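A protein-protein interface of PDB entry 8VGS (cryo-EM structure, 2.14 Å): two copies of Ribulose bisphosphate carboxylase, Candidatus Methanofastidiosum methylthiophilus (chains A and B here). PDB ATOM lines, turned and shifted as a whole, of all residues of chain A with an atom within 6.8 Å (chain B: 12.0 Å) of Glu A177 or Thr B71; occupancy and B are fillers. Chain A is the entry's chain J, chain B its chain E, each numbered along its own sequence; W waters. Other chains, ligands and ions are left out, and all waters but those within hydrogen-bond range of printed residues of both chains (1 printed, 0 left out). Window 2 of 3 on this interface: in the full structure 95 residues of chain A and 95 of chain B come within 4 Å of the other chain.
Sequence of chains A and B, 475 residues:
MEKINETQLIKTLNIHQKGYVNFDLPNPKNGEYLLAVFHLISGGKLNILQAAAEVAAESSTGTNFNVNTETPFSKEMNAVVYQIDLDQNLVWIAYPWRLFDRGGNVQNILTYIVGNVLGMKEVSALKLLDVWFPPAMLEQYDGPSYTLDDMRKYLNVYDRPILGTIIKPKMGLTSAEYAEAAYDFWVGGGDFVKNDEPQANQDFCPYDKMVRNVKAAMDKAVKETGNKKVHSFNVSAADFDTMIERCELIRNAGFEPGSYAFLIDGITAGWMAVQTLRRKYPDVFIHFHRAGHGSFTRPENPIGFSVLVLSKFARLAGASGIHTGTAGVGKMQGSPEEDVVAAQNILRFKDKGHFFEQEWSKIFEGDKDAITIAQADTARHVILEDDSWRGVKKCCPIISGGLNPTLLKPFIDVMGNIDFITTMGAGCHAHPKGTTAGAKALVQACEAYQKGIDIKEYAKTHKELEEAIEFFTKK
The side-chain hydroxyl (OH) of Tyr B20 lies within hydrogen-bond range of the side-chain hydroxyl (OG1) of Thr B61, at 2.9 Å.
The side-chain hydroxyl of Thr B61 lies within hydrogen-bond range of the side-chain amide oxygen of Asn B78, 2.5 Å away.
NZ of Lys B75 is in salt-bridge range of OE1 of Glu B70.
The side-chain hydroxyl of Thr B71 sits close to the backbone NH of Phe B73, 3.4 Å away.
The backbone NH of Ser B74 sits at hydrogen-bond distance from the side-chain hydroxyl of Thr B71 (2.9 Å).
The backbone carbonyl oxygen (O) of Ser B74 sits close to the side-chain amide oxygen (OD1) of Asn B78, at 3.3 Å.
Among the printed residues, pairs that only touch across the chains: Pro A169 with Thr B61 (3.2 Å), Pro A169 with Val B67 (3.7 Å), Pro A169 with Thr B69 (3.5 Å), Pro A169 with Glu B70 (3.7 Å), Pro A169 with Ser B74 (3.4 Å), Gly A172 with Phe B73 (3.2 Å), Gly A172 with Ser B74 (3.3 Å), Leu A173 with Thr B69 (3.5 Å), Leu A173 with Thr B71 (3.8 Å), Leu A173 with Ser B74 (3.8 Å) and Glu A177 with Thr B71 (3.9 Å).
Of chain B, only Thr B71 comes within 4 Å of Glu A177.
Of the printed residues of chain A, Thr B71 touches Leu A173 and Glu A177.
Of chain B, only Phe B73 and Ser B74 come within 4 Å of Gly A172.
Ser A175 touches none of the printed residues of chain B.
No residue of chain B comes within 4 Å of Ala A176.
No residue of chain B comes within 4 Å of Ala A179.
No residue of chain B comes within 4 Å of Ala A181.
Of the printed residues of chain A, Glu B70 touches Pro A169.
Of the printed residues of chain B, Pro A169 touches Thr B61 (3.2 Å), Val B67 (3.7 Å), Thr B69 (3.5 Å), Glu B70 (3.7 Å) and Ser B74 (3.4 Å).
Printed residues of chain A within 4 Å of Thr B61: Pro A169 (3.2 Å).
Asn B78 touches none of the printed residues of chain A.
Ser B60 touches none of the printed residues of chain A.
The nearest residue of chain B that does not touch Glu A177 is Thr B69 (5.8 Å).
The nearest residue of chain A that does not touch Thr B71 is Gly A172 (4.3 Å).
The nearest printed residue of chain B that does not touch Pro A169 is Thr B71 (4.8 Å).
Of the 24 printed residues of chain B, 7 touch a printed residue of chain A.
Hydrophobic or aromatic side chains of chain B that line the printed part of chain A: Val B67 and Phe B73.
Among the printed residues, 11 pairs touch across the chains.
No position is printed for both chains.
Of the 11 pairs that touch across the chains among the printed residues, none has its exchanged pair printed and touching as well.
Water W1 lies within hydrogen-bond range of OE1 of Glu A177 (2.5 Å), O of Gly A172 (2.8 Å), OG1 of Thr B71 (2.9 Å) and N of Thr A174 (3.4 Å).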
ATOM      1  N   ILE A 167       1.923   7.242  -0.822  1.00  0.00           N
ATOM      2  CA  ILE A 167       1.290   6.394  -1.826  1.00  0.00           C
ATOM      3  C   ILE A 167      -0.200   6.306  -1.515  1.00  0.00           C
ATOM      4  O   ILE A 167      -0.604   5.708  -0.517  1.00  0.00           O
ATOM      5  CB  ILE A 167       1.930   5.004  -1.874  1.00  0.00           C
ATOM      6  CG1 ILE A 167       3.410   5.117  -2.241  1.00  0.00           C
ATOM      7  CG2 ILE A 167       1.191   4.115  -2.864  1.00  0.00           C
ATOM      8  CD1 ILE A 167       3.668   5.922  -3.490  1.00  0.00           C
ATOM      9  N   PRO A 169      -3.981   4.947  -2.936  1.00  0.00           N
ATOM     10  CA  PRO A 169      -4.780   4.938  -1.694  1.00  0.00           C
ATOM     11  C   PRO A 169      -3.976   4.631  -0.433  1.00  0.00           C
ATOM     12  O   PRO A 169      -2.909   4.027  -0.504  1.00  0.00           O
ATOM     13  CB  PRO A 169      -5.819   3.834  -1.958  1.00  0.00           C
ATOM     14  CG  PRO A 169      -5.895   3.719  -3.448  1.00  0.00           C
ATOM     15  CD  PRO A 169      -4.490   3.966  -3.908  1.00  0.00           C
ATOM     16  N   GLY A 172      -5.257  -0.761   0.879  1.00  0.00           N
ATOM     17  CA  GLY A 172      -5.946  -1.522  -0.143  1.00  0.00           C
ATOM     18  C   GLY A 172      -5.091  -1.907  -1.329  1.00  0.00           C
ATOM     19  O   GLY A 172      -5.485  -2.801  -2.086  1.00  0.00           O
ATOM     20  N   LEU A 173      -3.943  -1.268  -1.519  1.00  0.00           N
ATOM     21  CA  LEU A 173      -3.022  -1.673  -2.568  1.00  0.00           C
ATOM     22  C   LEU A 173      -2.255  -2.920  -2.150  1.00  0.00           C
ATOM     23  O   LEU A 173      -1.902  -3.098  -0.981  1.00  0.00           O
ATOM     24  CB  LEU A 173      -2.037  -0.549  -2.889  1.00  0.00           C
ATOM     25  CG  LEU A 173      -2.594   0.708  -3.554  1.00  0.00           C
ATOM     26  CD1 LEU A 173      -1.460   1.619  -3.993  1.00  0.00           C
ATOM     27  CD2 LEU A 173      -3.474   0.335  -4.733  1.00  0.00           C
ATOM     28  N   THR A 174      -2.003  -3.792  -3.120  1.00  0.00           N
ATOM     29  CA  THR A 174      -1.132  -4.925  -2.868  1.00  0.00           C
ATOM     30  C   THR A 174       0.317  -4.453  -2.780  1.00  0.00           C
ATOM     31  O   THR A 174       0.632  -3.283  -3.015  1.00  0.00           O
ATOM     32  CB  THR A 174      -1.290  -5.986  -3.959  1.00  0.00           C
ATOM     33  OG1 THR A 174      -0.713  -5.515  -5.182  1.00  0.00           O
ATOM     34  CG2 THR A 174      -2.762  -6.304  -4.184  1.00  0.00           C
ATOM     35  N   SER A 175       1.204  -5.380  -2.411  1.00  0.00           N
ATOM     36  CA  SER A 175       2.626  -5.053  -2.342  1.00  0.00           C
ATOM     37  C   SER A 175       3.163  -4.654  -3.710  1.00  0.00           C
ATOM     38  O   SER A 175       3.944  -3.700  -3.827  1.00  0.00           O
ATOM     39  CB  SER A 175       3.409  -6.240  -1.782  1.00  0.00           C
ATOM     40  OG  SER A 175       3.295  -6.302  -0.372  1.00  0.00           O
ATOM     41  N   ALA A 176       2.738  -5.362  -4.757  1.00  0.00           N
ATOM     42  CA  ALA A 176       3.177  -5.038  -6.110  1.00  0.00           C
ATOM     43  C   ALA A 176       2.670  -3.668  -6.543  1.00  0.00           C
ATOM     44  O   ALA A 176       3.419  -2.874  -7.121  1.00  0.00           O
ATOM     45  CB  ALA A 176       2.704  -6.116  -7.081  1.00  0.00           C
ATOM     46  N   GLU A 177       1.394  -3.376  -6.277  1.00  0.00           N
ATOM     47  CA  GLU A 177       0.838  -2.079  -6.653  1.00  0.00           C
ATOM     48  C   GLU A 177       1.506  -0.944  -5.887  1.00  0.00           C
ATOM     49  O   GLU A 177       1.788   0.117  -6.459  1.00  0.00           O
ATOM     50  CB  GLU A 177      -0.672  -2.065  -6.418  1.00  0.00           C
ATOM     51  CG  GLU A 177      -1.489  -2.585  -7.590  1.00  0.00           C
ATOM     52  CD  GLU A 177      -2.623  -3.490  -7.150  1.00  0.00           C
ATOM     53  OE1 GLU A 177      -2.829  -3.633  -5.927  1.00  0.00           O
ATOM     54  OE2 GLU A 177      -3.310  -4.054  -8.026  1.00  0.00           O
ATOM     55  N   TYR A 178       1.758  -1.146  -4.592  1.00  0.00           N
ATOM     56  CA  TYR A 178       2.438  -0.130  -3.795  1.00  0.00           C
ATOM     57  C   TYR A 178       3.847   0.121  -4.319  1.00  0.00           C
ATOM     58  O   TYR A 178       4.279   1.274  -4.447  1.00  0.00           O
ATOM     59  CB  TYR A 178       2.476  -0.554  -2.325  1.00  0.00           C
ATOM     60  CG  TYR A 178       3.243   0.402  -1.446  1.00  0.00           C
ATOM     61  CD1 TYR A 178       2.656   1.573  -0.994  1.00  0.00           C
ATOM     62  CD2 TYR A 178       4.557   0.142  -1.077  1.00  0.00           C
ATOM     63  CE1 TYR A 178       3.349   2.454  -0.196  1.00  0.00           C
ATOM     64  CE2 TYR A 178       5.260   1.021  -0.285  1.00  0.00           C
ATOM     65  CZ  TYR A 178       4.652   2.178   0.149  1.00  0.00           C
ATOM     66  OH  TYR A 178       5.342   3.057   0.948  1.00  0.00           O
ATOM     67  N   ALA A 179       4.584  -0.954  -4.621  1.00  0.00           N
ATOM     68  CA  ALA A 179       5.928  -0.798  -5.164  1.00  0.00           C
ATOM     69  C   ALA A 179       5.897  -0.115  -6.525  1.00  0.00           C
ATOM     70  O   ALA A 179       6.782   0.685  -6.846  1.00  0.00           O
ATOM     71  CB  ALA A 179       6.617  -2.160  -5.258  1.00  0.00           C
ATOM     72  N   GLU A 180       4.880  -0.414  -7.337  1.00  0.00           N
ATOM     73  CA  GLU A 180       4.751   0.228  -8.640  1.00  0.00           C
ATOM     74  C   GLU A 180       4.489   1.722  -8.495  1.00  0.00           C
ATOM     75  O   GLU A 180       5.060   2.531  -9.233  1.00  0.00           O
ATOM     76  CB  GLU A 180       3.635  -0.440  -9.443  1.00  0.00           C
ATOM     77  CG  GLU A 180       3.414   0.161 -10.820  1.00  0.00           C
ATOM     78  CD  GLU A 180       4.582  -0.084 -11.752  1.00  0.00           C
ATOM     79  OE1 GLU A 180       5.311  -1.076 -11.544  1.00  0.00           O
ATOM     80  OE2 GLU A 180       4.768   0.712 -12.697  1.00  0.00           O
ATOM     81  N   ALA A 181       3.630   2.107  -7.547  1.00  0.00           N
ATOM     82  CA  ALA A 181       3.381   3.527  -7.305  1.00  0.00           C
ATOM     83  C   ALA A 181       4.634   4.229  -6.793  1.00  0.00           C
ATOM     84  O   ALA A 181       4.933   5.364  -7.196  1.00  0.00           O
ATOM     85  CB  ALA A 181       2.227   3.696  -6.319  1.00  0.00           C
ATOM     86  N   ALA A 182       5.379   3.568  -5.901  1.00  0.00           N
ATOM     87  CA  ALA A 182       6.621   4.145  -5.396  1.00  0.00           C
ATOM     88  C   ALA A 182       7.637   4.335  -6.516  1.00  0.00           C
ATOM     89  O   ALA A 182       8.292   5.381  -6.598  1.00  0.00           O
ATOM     90  CB  ALA A 182       7.199   3.264  -4.288  1.00  0.00           C
ATOM     91  N   ASN A 213       9.460  -5.828  -2.716  1.00  0.00           N
ATOM     92  CA  ASN A 213       9.004  -5.161  -3.929  1.00  0.00           C
ATOM     93  C   ASN A 213       9.456  -3.707  -3.959  1.00  0.00           C
ATOM     94  O   ASN A 213       9.814  -3.185  -5.019  1.00  0.00           O
ATOM     95  CB  ASN A 213       7.484  -5.264  -4.038  1.00  0.00           C
ATOM     96  CG  ASN A 213       7.018  -6.674  -4.351  1.00  0.00           C
ATOM     97  OD1 ASN A 213       7.828  -7.563  -4.612  1.00  0.00           O
ATOM     98  ND2 ASN A 213       5.708  -6.887  -4.322  1.00  0.00           N
ATOM     99  N   HIS B  16     -15.946  11.427  -5.276  1.00  0.00           N
ATOM    100  CA  HIS B  16     -15.017  10.843  -4.314  1.00  0.00           C
ATOM    101  C   HIS B  16     -15.701  10.544  -2.986  1.00  0.00           C
ATOM    102  O   HIS B  16     -15.440   9.508  -2.365  1.00  0.00           O
ATOM    103  CB  HIS B  16     -13.825  11.775  -4.103  1.00  0.00           C
ATOM    104  CG  HIS B  16     -13.061  11.497  -2.846  1.00  0.00           C
ATOM    105  ND1 HIS B  16     -12.307  10.358  -2.672  1.00  0.00           N
ATOM    106  CD2 HIS B  16     -12.936  12.211  -1.702  1.00  0.00           C
ATOM    107  CE1 HIS B  16     -11.751  10.379  -1.474  1.00  0.00           C
ATOM    108  NE2 HIS B  16     -12.115  11.494  -0.866  1.00  0.00           N
ATOM    109  N   GLY B  19     -18.014   7.284  -2.561  1.00  0.00           N
ATOM    110  CA  GLY B  19     -17.392   5.985  -2.376  1.00  0.00           C
ATOM    111  C   GLY B  19     -17.150   5.617  -0.928  1.00  0.00           C
ATOM    112  O   GLY B  19     -16.835   4.458  -0.639  1.00  0.00           O
ATOM    113  N   TYR B  20     -17.290   6.574  -0.011  1.00  0.00           N
ATOM    114  CA  TYR B  20     -17.120   6.334   1.415  1.00  0.00           C
ATOM    115  C   TYR B  20     -18.424   6.500   2.187  1.00  0.00           C
ATOM    116  O   TYR B  20     -18.403   6.627   3.414  1.00  0.00           O
ATOM    117  CB  TYR B  20     -16.040   7.259   1.981  1.00  0.00           C
ATOM    118  CG  TYR B  20     -14.669   6.986   1.412  1.00  0.00           C
ATOM    119  CD1 TYR B  20     -13.825   6.052   2.000  1.00  0.00           C
ATOM    120  CD2 TYR B  20     -14.226   7.644   0.272  1.00  0.00           C
ATOM    121  CE1 TYR B  20     -12.574   5.796   1.478  1.00  0.00           C
ATOM    122  CE2 TYR B  20     -12.979   7.391  -0.257  1.00  0.00           C
ATOM    123  CZ  TYR B  20     -12.157   6.467   0.349  1.00  0.00           C
ATOM    124  OH  TYR B  20     -10.913   6.212  -0.178  1.00  0.00           O
ATOM    125  N   SER B  60      -9.711   5.342   6.407  1.00  0.00           N
ATOM    126  CA  SER B  60      -9.636   3.990   5.853  1.00  0.00           C
ATOM    127  C   SER B  60      -8.654   3.875   4.693  1.00  0.00           C
ATOM    128  O   SER B  60      -7.661   3.154   4.813  1.00  0.00           O
ATOM    129  CB  SER B  60     -11.032   3.532   5.432  1.00  0.00           C
ATOM    130  OG  SER B  60     -11.555   4.366   4.415  1.00  0.00           O
ATOM    131  N   THR B  61      -8.889   4.560   3.574  1.00  0.00           N
ATOM    132  CA  THR B  61      -8.101   4.305   2.368  1.00  0.00           C
ATOM    133  C   THR B  61      -7.739   5.537   1.557  1.00  0.00           C
ATOM    134  O   THR B  61      -6.748   5.487   0.820  1.00  0.00           O
ATOM    135  CB  THR B  61      -8.837   3.324   1.441  1.00  0.00           C
ATOM    136  OG1 THR B  61     -10.169   3.793   1.197  1.00  0.00           O
ATOM    137  CG2 THR B  61      -8.888   1.925   2.045  1.00  0.00           C
ATOM    138  N   GLY B  62      -8.485   6.638   1.646  1.00  0.00           N
ATOM    139  CA  GLY B  62      -8.414   7.697   0.670  1.00  0.00           C
ATOM    140  C   GLY B  62      -7.832   8.992   1.201  1.00  0.00           C
ATOM    141  O   GLY B  62      -7.227   9.056   2.272  1.00  0.00           O
ATOM    142  N   THR B  63      -8.037  10.042   0.415  1.00  0.00           N
ATOM    143  CA  THR B  63      -7.507  11.373   0.685  1.00  0.00           C
ATOM    144  C   THR B  63      -8.602  12.365   0.300  1.00  0.00           C
ATOM    145  O   THR B  63      -9.773  12.002   0.156  1.00  0.00           O
ATOM    146  CB  THR B  63      -6.186  11.593  -0.070  1.00  0.00           C
ATOM    147  OG1 THR B  63      -5.465  10.356  -0.142  1.00  0.00           O
ATOM    148  CG2 THR B  63      -5.323  12.612   0.652  1.00  0.00           C
ATOM    149  N   PHE B  65      -8.959  13.706  -2.520  1.00  0.00           N
ATOM    150  CA  PHE B  65      -9.308  13.502  -3.920  1.00  0.00           C
ATOM    151  C   PHE B  65      -9.310  12.013  -4.240  1.00  0.00           C
ATOM    152  O   PHE B  65      -8.869  11.180  -3.444  1.00  0.00           O
ATOM    153  CB  PHE B  65      -8.333  14.228  -4.858  1.00  0.00           C
ATOM    154  CG  PHE B  65      -8.433  15.724  -4.804  1.00  0.00           C
ATOM    155  CD1 PHE B  65      -9.500  16.385  -5.390  1.00  0.00           C
ATOM    156  CD2 PHE B  65      -7.449  16.473  -4.179  1.00  0.00           C
ATOM    157  CE1 PHE B  65      -9.589  17.763  -5.345  1.00  0.00           C
ATOM    158  CE2 PHE B  65      -7.532  17.851  -4.131  1.00  0.00           C
ATOM    159  CZ  PHE B  65      -8.603  18.497  -4.714  1.00  0.00           C
ATOM    160  N   ASN B  66      -9.816  11.685  -5.427  1.00  0.00           N
ATOM    161  CA  ASN B  66      -9.671  10.344  -5.982  1.00  0.00           C
ATOM    162  C   ASN B  66      -8.320  10.240  -6.678  1.00  0.00           C
ATOM    163  O   ASN B  66      -8.012  11.042  -7.567  1.00  0.00           O
ATOM    164  CB  ASN B  66     -10.796  10.033  -6.966  1.00  0.00           C
ATOM    165  CG  ASN B  66     -12.115   9.746  -6.282  1.00  0.00           C
ATOM    166  OD1 ASN B  66     -13.148  10.305  -6.646  1.00  0.00           O
ATOM    167  ND2 ASN B  66     -12.090   8.861  -5.293  1.00  0.00           N
ATOM    168  N   VAL B  67      -7.522   9.262  -6.284  1.00  0.00           N
ATOM    169  CA  VAL B  67      -6.213   9.050  -6.890  1.00  0.00           C
ATOM    170  C   VAL B  67      -6.343   8.017  -7.999  1.00  0.00           C
ATOM    171  O   VAL B  67      -7.175   7.106  -7.939  1.00  0.00           O
ATOM    172  CB  VAL B  67      -5.174   8.622  -5.833  1.00  0.00           C
ATOM    173  CG1 VAL B  67      -4.823   9.799  -4.937  1.00  0.00           C
ATOM    174  CG2 VAL B  67      -5.694   7.452  -5.015  1.00  0.00           C
ATOM    175  N   ASN B  68      -5.505   8.160  -9.029  1.00  0.00           N
ATOM    176  CA  ASN B  68      -5.548   7.260 -10.176  1.00  0.00           C
ATOM    177  C   ASN B  68      -5.009   5.870  -9.864  1.00  0.00           C
ATOM    178  O   ASN B  68      -5.186   4.960 -10.680  1.00  0.00           O
ATOM    179  CB  ASN B  68      -4.770   7.868 -11.345  1.00  0.00           C
ATOM    180  CG  ASN B  68      -3.267   7.808 -11.143  1.00  0.00           C
ATOM    181  OD1 ASN B  68      -2.622   6.809 -11.463  1.00  0.00           O
ATOM    182  ND2 ASN B  68      -2.700   8.884 -10.608  1.00  0.00           N
ATOM    183  N   THR B  69      -4.363   5.682  -8.715  1.00  0.00           N
ATOM    184  CA  THR B  69      -3.894   4.368  -8.294  1.00  0.00           C
ATOM    185  C   THR B  69      -4.981   3.546  -7.617  1.00  0.00           C
ATOM    186  O   THR B  69      -4.708   2.416  -7.198  1.00  0.00           O
ATOM    187  CB  THR B  69      -2.701   4.512  -7.347  1.00  0.00           C
ATOM    188  OG1 THR B  69      -2.868   5.684  -6.540  1.00  0.00           O
ATOM    189  CG2 THR B  69      -1.407   4.627  -8.134  1.00  0.00           C
ATOM    190  N   GLU B  70      -6.192   4.085  -7.493  1.00  0.00           N
ATOM    191  CA  GLU B  70      -7.278   3.378  -6.827  1.00  0.00           C
ATOM    192  C   GLU B  70      -7.681   2.149  -7.633  1.00  0.00           C
ATOM    193  O   GLU B  70      -8.048   2.258  -8.807  1.00  0.00           O
ATOM    194  CB  GLU B  70      -8.474   4.309  -6.641  1.00  0.00           C
ATOM    195  CG  GLU B  70      -9.614   3.701  -5.839  1.00  0.00           C
ATOM    196  CD  GLU B  70     -10.844   4.590  -5.808  1.00  0.00           C
ATOM    197  OE1 GLU B  70     -11.364   4.927  -6.892  1.00  0.00           O
ATOM    198  OE2 GLU B  70     -11.292   4.949  -4.699  1.00  0.00           O
ATOM    199  N   THR B  71      -7.613   0.988  -7.003  1.00  0.00           N
ATOM    200  CA  THR B  71      -8.062  -0.260  -7.592  1.00  0.00           C
ATOM    201  C   THR B  71      -9.462  -0.602  -7.105  1.00  0.00           C
ATOM    202  O   THR B  71      -9.929  -0.065  -6.096  1.00  0.00           O
ATOM    203  CB  THR B  71      -7.098  -1.389  -7.234  1.00  0.00           C
ATOM    204  OG1 THR B  71      -7.251  -1.728  -5.850  1.00  0.00           O
ATOM    205  CG2 THR B  71      -5.660  -0.966  -7.491  1.00  0.00           C
ATOM    206  N   PRO B  72     -10.173  -1.478  -7.819  1.00  0.00           N
ATOM    207  CA  PRO B  72     -11.459  -1.966  -7.294  1.00  0.00           C
ATOM    208  C   PRO B  72     -11.316  -2.699  -5.972  1.00  0.00           C
ATOM    209  O   PRO B  72     -12.226  -2.639  -5.136  1.00  0.00           O
ATOM    210  CB  PRO B  72     -11.970  -2.892  -8.408  1.00  0.00           C
ATOM    211  CG  PRO B  72     -10.765  -3.232  -9.225  1.00  0.00           C
ATOM    212  CD  PRO B  72      -9.838  -2.064  -9.127  1.00  0.00           C
ATOM    213  N   PHE B  73     -10.193  -3.387  -5.758  1.00  0.00           N
ATOM    214  CA  PHE B  73      -9.940  -4.013  -4.466  1.00  0.00           C
ATOM    215  C   PHE B  73      -9.769  -2.974  -3.365  1.00  0.00           C
ATOM    216  O   PHE B  73     -10.178  -3.211  -2.223  1.00  0.00           O
ATOM    217  CB  PHE B  73      -8.703  -4.909  -4.552  1.00  0.00           C
ATOM    218  CG  PHE B  73      -8.448  -5.720  -3.311  1.00  0.00           C
ATOM    219  CD1 PHE B  73      -9.100  -6.924  -3.110  1.00  0.00           C
ATOM    220  CD2 PHE B  73      -7.545  -5.285  -2.355  1.00  0.00           C
ATOM    221  CE1 PHE B  73      -8.865  -7.675  -1.974  1.00  0.00           C
ATOM    222  CE2 PHE B  73      -7.305  -6.032  -1.217  1.00  0.00           C
ATOM    223  CZ  PHE B  73      -7.966  -7.229  -1.026  1.00  0.00           C
ATOM    224  N   SER B  74      -9.161  -1.828  -3.686  1.00  0.00           N
ATOM    225  CA  SER B  74      -8.980  -0.772  -2.694  1.00  0.00           C
ATOM    226  C   SER B  74     -10.318  -0.215  -2.227  1.00  0.00           C
ATOM    227  O   SER B  74     -10.482   0.116  -1.046  1.00  0.00           O
ATOM    228  CB  SER B  74      -8.105   0.342  -3.268  1.00  0.00           C
ATOM    229  OG  SER B  74      -7.076   0.701  -2.365  1.00  0.00           O
ATOM    230  N   LYS B  75     -11.287  -0.099  -3.138  1.00  0.00           N
ATOM    231  CA  LYS B  75     -12.604   0.407  -2.763  1.00  0.00           C
ATOM    232  C   LYS B  75     -13.327  -0.539  -1.812  1.00  0.00           C
ATOM    233  O   LYS B  75     -14.193  -0.100  -1.048  1.00  0.00           O
ATOM    234  CB  LYS B  75     -13.449   0.657  -4.012  1.00  0.00           C
ATOM    235  CG  LYS B  75     -12.757   1.495  -5.075  1.00  0.00           C
ATOM    236  CD  LYS B  75     -13.754   2.357  -5.831  1.00  0.00           C
ATOM    237  CE  LYS B  75     -13.671   2.120  -7.329  1.00  0.00           C
ATOM    238  NZ  LYS B  75     -12.716   3.055  -7.984  1.00  0.00           N
ATOM    239  N   GLU B  76     -12.995  -1.832  -1.844  1.00  0.00           N
ATOM    240  CA  GLU B  76     -13.595  -2.767  -0.898  1.00  0.00           C
ATOM    241  C   GLU B  76     -13.151  -2.480   0.531  1.00  0.00           C
ATOM    242  O   GLU B  76     -13.891  -2.765   1.479  1.00  0.00           O
ATOM    243  CB  GLU B  76     -13.251  -4.206  -1.284  1.00  0.00           C
ATOM    244  CG  GLU B  76     -13.709  -4.609  -2.677  1.00  0.00           C
ATOM    245  CD  GLU B  76     -15.122  -4.151  -2.987  1.00  0.00           C
ATOM    246  OE1 GLU B  76     -15.986  -4.224  -2.089  1.00  0.00           O
ATOM    247  OE2 GLU B  76     -15.368  -3.718  -4.131  1.00  0.00           O
ATOM    248  N   MET B  77     -11.958  -1.916   0.705  1.00  0.00           N
ATOM    249  CA  MET B  77     -11.460  -1.542   2.022  1.00  0.00           C
ATOM    250  C   MET B  77     -11.931  -0.164   2.461  1.00  0.00           C
ATOM    251  O   MET B  77     -11.521   0.301   3.530  1.00  0.00           O
ATOM    252  CB  MET B  77      -9.931  -1.596   2.039  1.00  0.00           C
ATOM    253  CG  MET B  77      -9.350  -2.916   1.559  1.00  0.00           C
ATOM    254  SD  MET B  77      -9.514  -4.234   2.776  1.00  0.00           S
ATOM    255  CE  MET B  77     -11.158  -4.841   2.407  1.00  0.00           C
ATOM    256  N   ASN B  78     -12.767   0.496   1.663  1.00  0.00           N
ATOM    257  CA  ASN B  78     -13.281   1.811   2.019  1.00  0.00           C
ATOM    258  C   ASN B  78     -14.136   1.740   3.277  1.00  0.00           C
ATOM    259  O   ASN B  78     -15.008   0.879   3.409  1.00  0.00           O
ATOM    260  CB  ASN B  78     -14.116   2.377   0.870  1.00  0.00           C
ATOM    261  CG  ASN B  78     -13.269   2.982  -0.227  1.00  0.00           C
ATOM    262  OD1 ASN B  78     -12.041   2.935  -0.181  1.00  0.00           O
ATOM    263  ND2 ASN B  78     -13.925   3.565  -1.222  1.00  0.00           N
ATOM    264  N   ALA B  79     -13.876   2.650   4.211  1.00  0.00           N
ATOM    265  CA  ALA B  79     -14.825   2.888   5.288  1.00  0.00           C
ATOM    266  C   ALA B  79     -16.034   3.630   4.735  1.00  0.00           C
ATOM    267  O   ALA B  79     -15.900   4.520   3.892  1.00  0.00           O
ATOM    268  CB  ALA B  79     -14.178   3.688   6.416  1.00  0.00           C
ATOM    269  N   ARG B  98     -10.114  -5.790   7.925  1.00  0.00           N
ATOM    270  CA  ARG B  98      -9.024  -6.151   7.026  1.00  0.00           C
ATOM    271  C   ARG B  98      -8.007  -5.025   6.873  1.00  0.00           C
ATOM    272  O   ARG B  98      -6.824  -5.290   6.631  1.00  0.00           O
ATOM    273  CB  ARG B  98      -9.598  -6.524   5.659  1.00  0.00           C
ATOM    274  CG  ARG B  98      -8.747  -7.476   4.859  1.00  0.00           C
ATOM    275  CD  ARG B  98      -9.594  -8.519   4.153  1.00  0.00           C
ATOM    276  NE  ARG B  98      -8.806  -9.278   3.190  1.00  0.00           N
ATOM    277  CZ  ARG B  98      -9.173  -9.510   1.939  1.00  0.00           C
ATOM    278  NH1 ARG B  98     -10.323  -9.063   1.461  1.00  0.00           N
ATOM    279  NH2 ARG B  98      -8.364 -10.204   1.145  1.00  0.00           N
ATOM    280  N   LEU B  99      -8.453  -3.765   6.981  1.00  0.00           N
ATOM    281  CA  LEU B  99      -7.539  -2.625   6.957  1.00  0.00           C
ATOM    282  C   LEU B  99      -6.482  -2.716   8.049  1.00  0.00           C
ATOM    283  O   LEU B  99      -5.331  -2.327   7.831  1.00  0.00           O
ATOM    284  CB  LEU B  99      -8.322  -1.322   7.120  1.00  0.00           C
ATOM    285  CG  LEU B  99      -9.253  -0.862   6.000  1.00  0.00           C
ATOM    286  CD1 LEU B  99     -10.299   0.092   6.552  1.00  0.00           C
ATOM    287  CD2 LEU B  99      -8.460  -0.198   4.892  1.00  0.00           C
HETATM  288  O   HOH W   1      -4.970  -3.209  -4.773  1.00  0.00           O
